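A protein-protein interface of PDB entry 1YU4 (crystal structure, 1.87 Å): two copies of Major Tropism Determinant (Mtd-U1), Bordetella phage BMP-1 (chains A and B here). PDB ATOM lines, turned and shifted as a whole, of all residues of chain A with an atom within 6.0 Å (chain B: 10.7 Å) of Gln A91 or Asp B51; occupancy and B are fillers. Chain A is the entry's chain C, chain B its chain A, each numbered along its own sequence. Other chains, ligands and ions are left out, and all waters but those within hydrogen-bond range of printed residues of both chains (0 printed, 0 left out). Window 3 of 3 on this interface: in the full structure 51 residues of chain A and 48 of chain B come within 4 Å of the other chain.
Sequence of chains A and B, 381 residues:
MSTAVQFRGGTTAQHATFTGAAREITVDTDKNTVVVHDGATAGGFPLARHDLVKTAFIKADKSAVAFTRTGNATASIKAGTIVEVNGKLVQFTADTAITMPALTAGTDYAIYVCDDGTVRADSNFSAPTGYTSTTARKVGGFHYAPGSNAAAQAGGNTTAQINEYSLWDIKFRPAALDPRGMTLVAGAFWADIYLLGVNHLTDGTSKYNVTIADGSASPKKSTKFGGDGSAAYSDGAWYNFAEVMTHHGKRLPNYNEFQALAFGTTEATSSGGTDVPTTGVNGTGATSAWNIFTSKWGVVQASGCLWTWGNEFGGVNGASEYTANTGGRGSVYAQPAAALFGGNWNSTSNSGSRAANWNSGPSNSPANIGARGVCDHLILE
The side-chain carboxylate (OD2) of Asp B51 lies close to the side-chain amide oxygen (OE1) of Gln A91 (3.4 Å).
The backbone carbonyl oxygen (O) of Ile A82 sits at hydrogen-bond distance from the backbone NH (N) of Ile A58.
Asp B51 touches Ile A58.
Leu B52 touches Ile A58.
Asp B51 touches Ile A82 (OD2 to CD1, 3.96 Å).
Lys B54 touches Ile A82.
CB of Asp B51 touches CD1 of Leu A89 (3.9 Å).
CD1 of Leu A89 touches CG of Leu B52, at 3.8 Å.
Printed residues of chain B within 4 Å of Ile A58: Asp B51 and Leu B52.
Of the printed residues of chain B, Ile A82 touches Asp B51 and Lys B54.
Of chain B, only Asp B51 (3.9 Å) and Leu B52 (3.8 Å) come within 4 Å of Leu A89.
No residue of chain B comes within 4 Å of Val A90.
Gln A91 touches just one residue of chain B: Asp B51 (3.4 Å).
No residue of chain B comes within 4 Å of Phe A92.
Of chain A, only Ile A58 (3.4 Å), Ile A82 (3.96 Å), Leu A89 (3.9 Å) and Gln A91 (3.4 Å) come within 4 Å of Asp B51.
Of the printed residues of chain A, Lys B54 touches Ile A82 (3.4 Å).
The nearest printed residue of chain A that does not touch Lys B54 is Ile A58 (4.2 Å).
Of the 18 printed residues of chain B, 3 touch a printed residue of chain A.
Hydrophobic or aromatic side chains of chain B within 4 Å of the printed part of chain A: Leu B52.
Along chain B the printed residues that touch a printed residue of chain A span positions 51 to 54.
Of the 10 printed residues of chain A, 4 touch a printed residue of chain B.
Hydrophobic or aromatic side chains of chain A within 4 Å of the printed part of chain B: Ile A58, Ile A82 and Leu A89.
Among the printed residues, no Asp or Glu carboxylate lies within 4 Å of a Lys or Arg side-chain nitrogen of the other chain.
No position is printed for both chains.
Of the 7 pairs that touch across the chains among the printed residues, none has its exchanged pair printed and touching as well.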
ATOM      1  N   ILE A  58       3.801  -0.335 -30.861  1.00  0.00           N
ATOM      2  CA  ILE A  58       3.928   0.542 -32.016  1.00  0.00           C
ATOM      3  C   ILE A  58       4.485  -0.237 -33.200  1.00  0.00           C
ATOM      4  O   ILE A  58       5.403  -1.037 -33.041  1.00  0.00           O
ATOM      5  CB  ILE A  58       4.863   1.730 -31.677  1.00  0.00           C
ATOM      6  CG1 ILE A  58       4.326   2.512 -30.474  1.00  0.00           C
ATOM      7  CG2 ILE A  58       5.017   2.656 -32.878  1.00  0.00           C
ATOM      8  CD1 ILE A  58       5.374   3.359 -29.784  1.00  0.00           C
ATOM      9  N   THR A  81       9.286  -2.349 -34.868  1.00  0.00           N
ATOM     10  CA  THR A  81       8.247  -2.781 -33.933  1.00  0.00           C
ATOM     11  C   THR A  81       8.739  -2.634 -32.493  1.00  0.00           C
ATOM     12  O   THR A  81       9.777  -3.182 -32.134  1.00  0.00           O
ATOM     13  CB  THR A  81       7.832  -4.244 -34.198  1.00  0.00           C
ATOM     14  OG1 THR A  81       7.391  -4.394 -35.554  1.00  0.00           O
ATOM     15  CG2 THR A  81       6.606  -4.626 -33.371  1.00  0.00           C
ATOM     16  N   ILE A  82       7.980  -1.894 -31.686  1.00  0.00           N
ATOM     17  CA  ILE A  82       8.319  -1.613 -30.293  1.00  0.00           C
ATOM     18  C   ILE A  82       7.216  -2.151 -29.390  1.00  0.00           C
ATOM     19  O   ILE A  82       6.044  -1.863 -29.606  1.00  0.00           O
ATOM     20  CB  ILE A  82       8.454  -0.091 -30.081  1.00  0.00           C
ATOM     21  CG1 ILE A  82       9.512   0.506 -31.020  1.00  0.00           C
ATOM     22  CG2 ILE A  82       8.799   0.226 -28.626  1.00  0.00           C
ATOM     23  CD1 ILE A  82       9.188   1.917 -31.457  1.00  0.00           C
ATOM     24  N   VAL A  83       7.599  -2.917 -28.373  1.00  0.00           N
ATOM     25  CA  VAL A  83       6.648  -3.596 -27.494  1.00  0.00           C
ATOM     26  C   VAL A  83       7.046  -3.440 -26.027  1.00  0.00           C
ATOM     27  O   VAL A  83       8.089  -3.937 -25.609  1.00  0.00           O
ATOM     28  CB  VAL A  83       6.569  -5.110 -27.811  1.00  0.00           C
ATOM     29  CG1 VAL A  83       5.417  -5.759 -27.052  1.00  0.00           C
ATOM     30  CG2 VAL A  83       6.435  -5.347 -29.314  1.00  0.00           C
ATOM     31  N   LEU A  89      11.458  -1.996 -22.430  1.00  0.00           N
ATOM     32  CA  LEU A  89      11.236  -1.546 -23.796  1.00  0.00           C
ATOM     33  C   LEU A  89      11.970  -2.495 -24.737  1.00  0.00           C
ATOM     34  O   LEU A  89      13.188  -2.423 -24.891  1.00  0.00           O
ATOM     35  CB  LEU A  89      11.721  -0.105 -23.975  1.00  0.00           C
ATOM     36  CG  LEU A  89      11.199   0.641 -25.206  1.00  0.00           C
ATOM     37  CD1 LEU A  89      11.317   2.144 -24.990  1.00  0.00           C
ATOM     38  CD2 LEU A  89      11.936   0.221 -26.478  1.00  0.00           C
ATOM     39  N   VAL A  90      11.213  -3.396 -25.352  1.00  0.00           N
ATOM     40  CA  VAL A  90      11.759  -4.379 -26.276  1.00  0.00           C
ATOM     41  C   VAL A  90      11.446  -3.932 -27.692  1.00  0.00           C
ATOM     42  O   VAL A  90      10.281  -3.793 -28.054  1.00  0.00           O
ATOM     43  CB  VAL A  90      11.141  -5.764 -26.027  1.00  0.00           C
ATOM     44  CG1 VAL A  90      11.672  -6.789 -27.030  1.00  0.00           C
ATOM     45  CG2 VAL A  90      11.410  -6.203 -24.595  1.00  0.00           C
ATOM     46  N   GLN A  91      12.483  -3.695 -28.490  1.00  0.00           N
ATOM     47  CA  GLN A  91      12.283  -3.290 -29.878  1.00  0.00           C
ATOM     48  C   GLN A  91      13.122  -4.116 -30.847  1.00  0.00           C
ATOM     49  O   GLN A  91      14.033  -4.838 -30.447  1.00  0.00           O
ATOM     50  CB  GLN A  91      12.529  -1.782 -30.044  1.00  0.00           C
ATOM     51  CG  GLN A  91      13.903  -1.371 -30.543  1.00  0.00           C
ATOM     52  CD  GLN A  91      14.093   0.130 -30.502  1.00  0.00           C
ATOM     53  OE1 GLN A  91      13.498   0.858 -31.304  1.00  0.00           O
ATOM     54  NE2 GLN A  91      14.908   0.604 -29.563  1.00  0.00           N
ATOM     55  N   PHE A  92      12.780  -4.004 -32.127  1.00  0.00           N
ATOM     56  CA  PHE A  92      13.412  -4.774 -33.189  1.00  0.00           C
ATOM     57  C   PHE A  92      13.749  -3.817 -34.321  1.00  0.00           C
ATOM     58  O   PHE A  92      12.864  -3.397 -35.065  1.00  0.00           O
ATOM     59  CB  PHE A  92      12.469  -5.870 -33.690  1.00  0.00           C
ATOM     60  CG  PHE A  92      11.971  -6.787 -32.610  1.00  0.00           C
ATOM     61  CD1 PHE A  92      12.676  -7.936 -32.278  1.00  0.00           C
ATOM     62  CD2 PHE A  92      10.796  -6.500 -31.926  1.00  0.00           C
ATOM     63  CE1 PHE A  92      12.220  -8.782 -31.285  1.00  0.00           C
ATOM     64  CE2 PHE A  92      10.333  -7.342 -30.929  1.00  0.00           C
ATOM     65  CZ  PHE A  92      11.046  -8.488 -30.607  1.00  0.00           C
ATOM     66  N   THR A  93      15.025  -3.458 -34.431  1.00  0.00           N
ATOM     67  CA  THR A  93      15.483  -2.496 -35.434  1.00  0.00           C
ATOM     68  C   THR A  93      15.496  -3.098 -36.840  1.00  0.00           C
ATOM     69  O   THR A  93      15.343  -2.376 -37.823  1.00  0.00           O
ATOM     70  CB  THR A  93      16.888  -1.948 -35.073  1.00  0.00           C
ATOM     71  OG1 THR A  93      17.787  -3.030 -34.786  1.00  0.00           O
ATOM     72  CG2 THR A  93      16.845  -1.153 -33.775  1.00  0.00           C
ATOM     73  N   GLY A 117      13.956  -9.738 -24.693  1.00  0.00           N
ATOM     74  CA  GLY A 117      14.210  -9.286 -26.054  1.00  0.00           C
ATOM     75  C   GLY A 117      13.919 -10.284 -27.166  1.00  0.00           C
ATOM     76  O   GLY A 117      14.095  -9.957 -28.342  1.00  0.00           O
ATOM     77  N   ASP B  30      19.367  -0.589 -17.309  1.00  0.00           N
ATOM     78  CA  ASP B  30      18.764  -1.500 -18.288  1.00  0.00           C
ATOM     79  C   ASP B  30      17.768  -0.761 -19.182  1.00  0.00           C
ATOM     80  O   ASP B  30      17.794  -0.912 -20.403  1.00  0.00           O
ATOM     81  CB  ASP B  30      18.045  -2.660 -17.590  1.00  0.00           C
ATOM     82  CG  ASP B  30      19.002  -3.659 -16.965  1.00  0.00           C
ATOM     83  OD1 ASP B  30      20.093  -3.896 -17.529  1.00  0.00           O
ATOM     84  OD2 ASP B  30      18.734  -4.274 -15.911  1.00  0.00           O
ATOM     85  N   LYS B  31      16.893   0.029 -18.559  1.00  0.00           N
ATOM     86  CA  LYS B  31      15.844   0.764 -19.262  1.00  0.00           C
ATOM     87  C   LYS B  31      16.345   2.084 -19.855  1.00  0.00           C
ATOM     88  O   LYS B  31      15.698   2.652 -20.738  1.00  0.00           O
ATOM     89  CB  LYS B  31      14.689   1.070 -18.304  1.00  0.00           C
ATOM     90  CG  LYS B  31      14.063  -0.147 -17.640  1.00  0.00           C
ATOM     91  CD  LYS B  31      12.726   0.213 -17.000  1.00  0.00           C
ATOM     92  CE  LYS B  31      12.410  -0.652 -15.788  1.00  0.00           C
ATOM     93  NZ  LYS B  31      12.342  -2.094 -16.118  1.00  0.00           N
ATOM     94  N   ASN B  32      17.493   2.564 -19.375  1.00  0.00           N
ATOM     95  CA  ASN B  32      17.984   3.906 -19.688  1.00  0.00           C
ATOM     96  C   ASN B  32      16.923   4.980 -19.450  1.00  0.00           C
ATOM     97  O   ASN B  32      16.623   5.792 -20.329  1.00  0.00           O
ATOM     98  CB  ASN B  32      18.515   3.977 -21.121  1.00  0.00           C
ATOM     99  CG  ASN B  32      19.801   3.207 -21.300  1.00  0.00           C
ATOM    100  OD1 ASN B  32      19.868   2.263 -22.086  1.00  0.00           O
ATOM    101  ND2 ASN B  32      20.832   3.604 -20.568  1.00  0.00           N
ATOM    102  N   THR B  33      16.353   4.965 -18.253  1.00  0.00           N
ATOM    103  CA  THR B  33      15.403   5.987 -17.847  1.00  0.00           C
ATOM    104  C   THR B  33      15.653   6.426 -16.406  1.00  0.00           C
ATOM    105  O   THR B  33      16.450   5.822 -15.693  1.00  0.00           O
ATOM    106  CB  THR B  33      13.958   5.466 -18.027  1.00  0.00           C
ATOM    107  OG1 THR B  33      13.033   6.551 -17.905  1.00  0.00           O
ATOM    108  CG2 THR B  33      13.562   4.488 -16.915  1.00  0.00           C
ATOM    109  N   LEU B  47      10.188   6.522 -15.164  1.00  0.00           N
ATOM    110  CA  LEU B  47       9.595   7.472 -16.093  1.00  0.00           C
ATOM    111  C   LEU B  47       9.626   6.874 -17.491  1.00  0.00           C
ATOM    112  O   LEU B  47      10.401   5.961 -17.771  1.00  0.00           O
ATOM    113  CB  LEU B  47      10.342   8.809 -16.070  1.00  0.00           C
ATOM    114  CG  LEU B  47      10.468   9.532 -14.722  1.00  0.00           C
ATOM    115  CD1 LEU B  47      11.036  10.926 -14.930  1.00  0.00           C
ATOM    116  CD2 LEU B  47       9.139   9.605 -13.988  1.00  0.00           C
ATOM    117  N   ALA B  48       8.778   7.409 -18.361  1.00  0.00           N
ATOM    118  CA  ALA B  48       8.576   6.873 -19.700  1.00  0.00           C
ATOM    119  C   ALA B  48       9.598   7.443 -20.669  1.00  0.00           C
ATOM    120  O   ALA B  48       9.878   8.640 -20.648  1.00  0.00           O
ATOM    121  CB  ALA B  48       7.168   7.203 -20.182  1.00  0.00           C
ATOM    122  N   ARG B  49      10.146   6.585 -21.520  1.00  0.00           N
ATOM    123  CA  ARG B  49      11.015   7.033 -22.604  1.00  0.00           C
ATOM    124  C   ARG B  49      10.165   7.562 -23.754  1.00  0.00           C
ATOM    125  O   ARG B  49       8.996   7.194 -23.885  1.00  0.00           O
ATOM    126  CB  ARG B  49      11.909   5.893 -23.084  1.00  0.00           C
ATOM    127  CG  ARG B  49      13.175   5.741 -22.258  1.00  0.00           C
ATOM    128  CD  ARG B  49      14.084   4.619 -22.718  1.00  0.00           C
ATOM    129  NE  ARG B  49      14.390   4.719 -24.142  1.00  0.00           N
ATOM    130  CZ  ARG B  49      15.030   3.790 -24.838  1.00  0.00           C
ATOM    131  NH1 ARG B  49      15.460   2.675 -24.252  1.00  0.00           N
ATOM    132  NH2 ARG B  49      15.249   3.978 -26.134  1.00  0.00           N
ATOM    133  N   HIS B  50      10.756   8.421 -24.583  1.00  0.00           N
ATOM    134  CA  HIS B  50      10.030   9.055 -25.683  1.00  0.00           C
ATOM    135  C   HIS B  50       9.648   8.071 -26.782  1.00  0.00           C
ATOM    136  O   HIS B  50       8.668   8.283 -27.493  1.00  0.00           O
ATOM    137  CB  HIS B  50      10.836  10.196 -26.306  1.00  0.00           C
ATOM    138  CG  HIS B  50      10.088  10.937 -27.372  1.00  0.00           C
ATOM    139  ND1 HIS B  50      10.711  11.606 -28.402  1.00  0.00           N
ATOM    140  CD2 HIS B  50       8.759  11.100 -27.571  1.00  0.00           C
ATOM    141  CE1 HIS B  50       9.797  12.156 -29.183  1.00  0.00           C
ATOM    142  NE2 HIS B  50       8.605  11.860 -28.704  1.00  0.00           N
ATOM    143  N   ASP B  51      10.428   7.006 -26.928  1.00  0.00           N
ATOM    144  CA  ASP B  51      10.164   5.995 -27.949  1.00  0.00           C
ATOM    145  C   ASP B  51       8.722   5.467 -27.891  1.00  0.00           C
ATOM    146  O   ASP B  51       8.115   5.204 -28.926  1.00  0.00           O
ATOM    147  CB  ASP B  51      11.160   4.830 -27.818  1.00  0.00           C
ATOM    148  CG  ASP B  51      11.895   4.532 -29.116  1.00  0.00           C
ATOM    149  OD1 ASP B  51      12.154   5.471 -29.905  1.00  0.00           O
ATOM    150  OD2 ASP B  51      12.258   3.376 -29.426  1.00  0.00           O
ATOM    151  N   LEU B  52       8.179   5.339 -26.682  1.00  0.00           N
ATOM    152  CA  LEU B  52       6.850   4.767 -26.479  1.00  0.00           C
ATOM    153  C   LEU B  52       5.701   5.694 -26.877  1.00  0.00           C
ATOM    154  O   LEU B  52       4.580   5.232 -27.082  1.00  0.00           O
ATOM    155  CB  LEU B  52       6.686   4.343 -25.019  1.00  0.00           C
ATOM    156  CG  LEU B  52       7.697   3.294 -24.544  1.00  0.00           C
ATOM    157  CD1 LEU B  52       7.632   3.111 -23.042  1.00  0.00           C
ATOM    158  CD2 LEU B  52       7.465   1.967 -25.258  1.00  0.00           C
ATOM    159  N   VAL B  53       5.968   6.993 -26.973  1.00  0.00           N
ATOM    160  CA  VAL B  53       4.940   7.964 -27.355  1.00  0.00           C
ATOM    161  C   VAL B  53       5.278   8.702 -28.644  1.00  0.00           C
ATOM    162  O   VAL B  53       4.751   9.787 -28.898  1.00  0.00           O
ATOM    163  CB  VAL B  53       4.649   8.990 -26.230  1.00  0.00           C
ATOM    164  CG1 VAL B  53       4.162   8.285 -24.988  1.00  0.00           C
ATOM    165  CG2 VAL B  53       5.870   9.841 -25.922  1.00  0.00           C
ATOM    166  N   LYS B  54       6.158   8.128 -29.458  1.00  0.00           N
ATOM    167  CA  LYS B  54       6.292   8.599 -30.824  1.00  0.00           C
ATOM    168  C   LYS B  54       5.032   8.140 -31.569  1.00  0.00           C
ATOM    169  O   LYS B  54       4.400   7.150 -31.178  1.00  0.00           O
ATOM    170  CB  LYS B  54       7.588   8.101 -31.484  1.00  0.00           C
ATOM    171  CG  LYS B  54       7.569   6.658 -31.986  1.00  0.00           C
ATOM    172  CD  LYS B  54       8.767   6.369 -32.901  1.00  0.00           C
ATOM    173  CE  LYS B  54       9.553   5.142 -32.456  1.00  0.00           C
ATOM    174  NZ  LYS B  54      10.171   4.427 -33.609  1.00  0.00           N
ATOM    175  N   THR B  55       4.683   8.852 -32.632  1.00  0.00           N
ATOM    176  CA  THR B  55       3.376   8.744 -33.295  1.00  0.00           C
ATOM    177  C   THR B  55       2.207   9.255 -32.443  1.00  0.00           C
ATOM    178  O   THR B  55       1.055   8.973 -32.760  1.00  0.00           O
ATOM    179  CB  THR B  55       3.067   7.296 -33.778  1.00  0.00           C
ATOM    180  OG1 THR B  55       2.595   6.500 -32.683  1.00  0.00           O
ATOM    181  CG2 THR B  55       4.319   6.575 -34.294  1.00  0.00           C
ATOM    182  N   ALA B  56       2.485  10.011 -31.381  1.00  0.00           N
ATOM    183  CA  ALA B  56       1.409  10.601 -30.583  1.00  0.00           C
ATOM    184  C   ALA B  56       0.673  11.652 -31.414  1.00  0.00           C
ATOM    185  O   ALA B  56       1.294  12.500 -32.044  1.00  0.00           O
ATOM    186  CB  ALA B  56       1.952  11.220 -29.308  1.00  0.00           C
ATOM    187  N   GLU B  84       3.271  14.677 -32.458  1.00  0.00           N
ATOM    188  CA  GLU B  84       4.684  14.302 -32.440  1.00  0.00           C
ATOM    189  C   GLU B  84       5.197  14.165 -33.870  1.00  0.00           C
ATOM    190  O   GLU B  84       4.611  13.447 -34.673  1.00  0.00           O
ATOM    191  CB  GLU B  84       4.878  12.978 -31.692  1.00  0.00           C
ATOM    192  CG  GLU B  84       6.329  12.661 -31.319  1.00  0.00           C
ATOM    193  CD  GLU B  84       7.014  11.659 -32.243  1.00  0.00           C
ATOM    194  OE1 GLU B  84       6.317  10.888 -32.944  1.00  0.00           O
ATOM    195  OE2 GLU B  84       8.269  11.633 -32.262  1.00  0.00           O
ATOM    196  N   ASN B  86       9.097  13.762 -35.647  1.00  0.00           N
ATOM    197  CA  ASN B  86      10.558  13.690 -35.651  1.00  0.00           C
ATOM    198  C   ASN B  86      11.184  14.169 -34.340  1.00  0.00           C
ATOM    199  O   ASN B  86      12.058  15.040 -34.333  1.00  0.00           O
ATOM    200  CB  ASN B  86      11.129  14.481 -36.835  1.00  0.00           C
ATOM    201  CG  ASN B  86      12.571  14.099 -37.157  1.00  0.00           C
ATOM    202  OD1 ASN B  86      12.980  12.953 -36.968  1.00  0.00           O
ATOM    203  ND2 ASN B  86      13.342  15.063 -37.643  1.00  0.00           N
ATOM    204  N   GLY B  87      10.715  13.607 -33.231  1.00  0.00           N
ATOM    205  CA  GLY B  87      11.214  13.975 -31.917  1.00  0.00           C
ATOM    206  C   GLY B  87      10.517  15.157 -31.253  1.00  0.00           C
ATOM    207  O   GLY B  87      10.510  15.255 -30.027  1.00  0.00           O
ATOM    208  N   LYS B  88       9.935  16.047 -32.055  1.00  0.00           N
ATOM    209  CA  LYS B  88       9.410  17.321 -31.564  1.00  0.00           C
ATOM    210  C   LYS B  88       7.927  17.255 -31.197  1.00  0.00           C
ATOM    211  O   LYS B  88       7.125  16.651 -31.905  1.00  0.00           O
ATOM    212  CB  LYS B  88       9.601  18.417 -32.620  1.00  0.00           C
ATOM    213  CG  LYS B  88      10.994  19.052 -32.656  1.00  0.00           C
ATOM    214  CD  LYS B  88      10.918  20.564 -32.911  1.00  0.00           C
ATOM    215  CE  LYS B  88      12.005  21.052 -33.855  1.00  0.00           C
ATOM    216  NZ  LYS B  88      11.826  22.495 -34.193  1.00  0.00           N
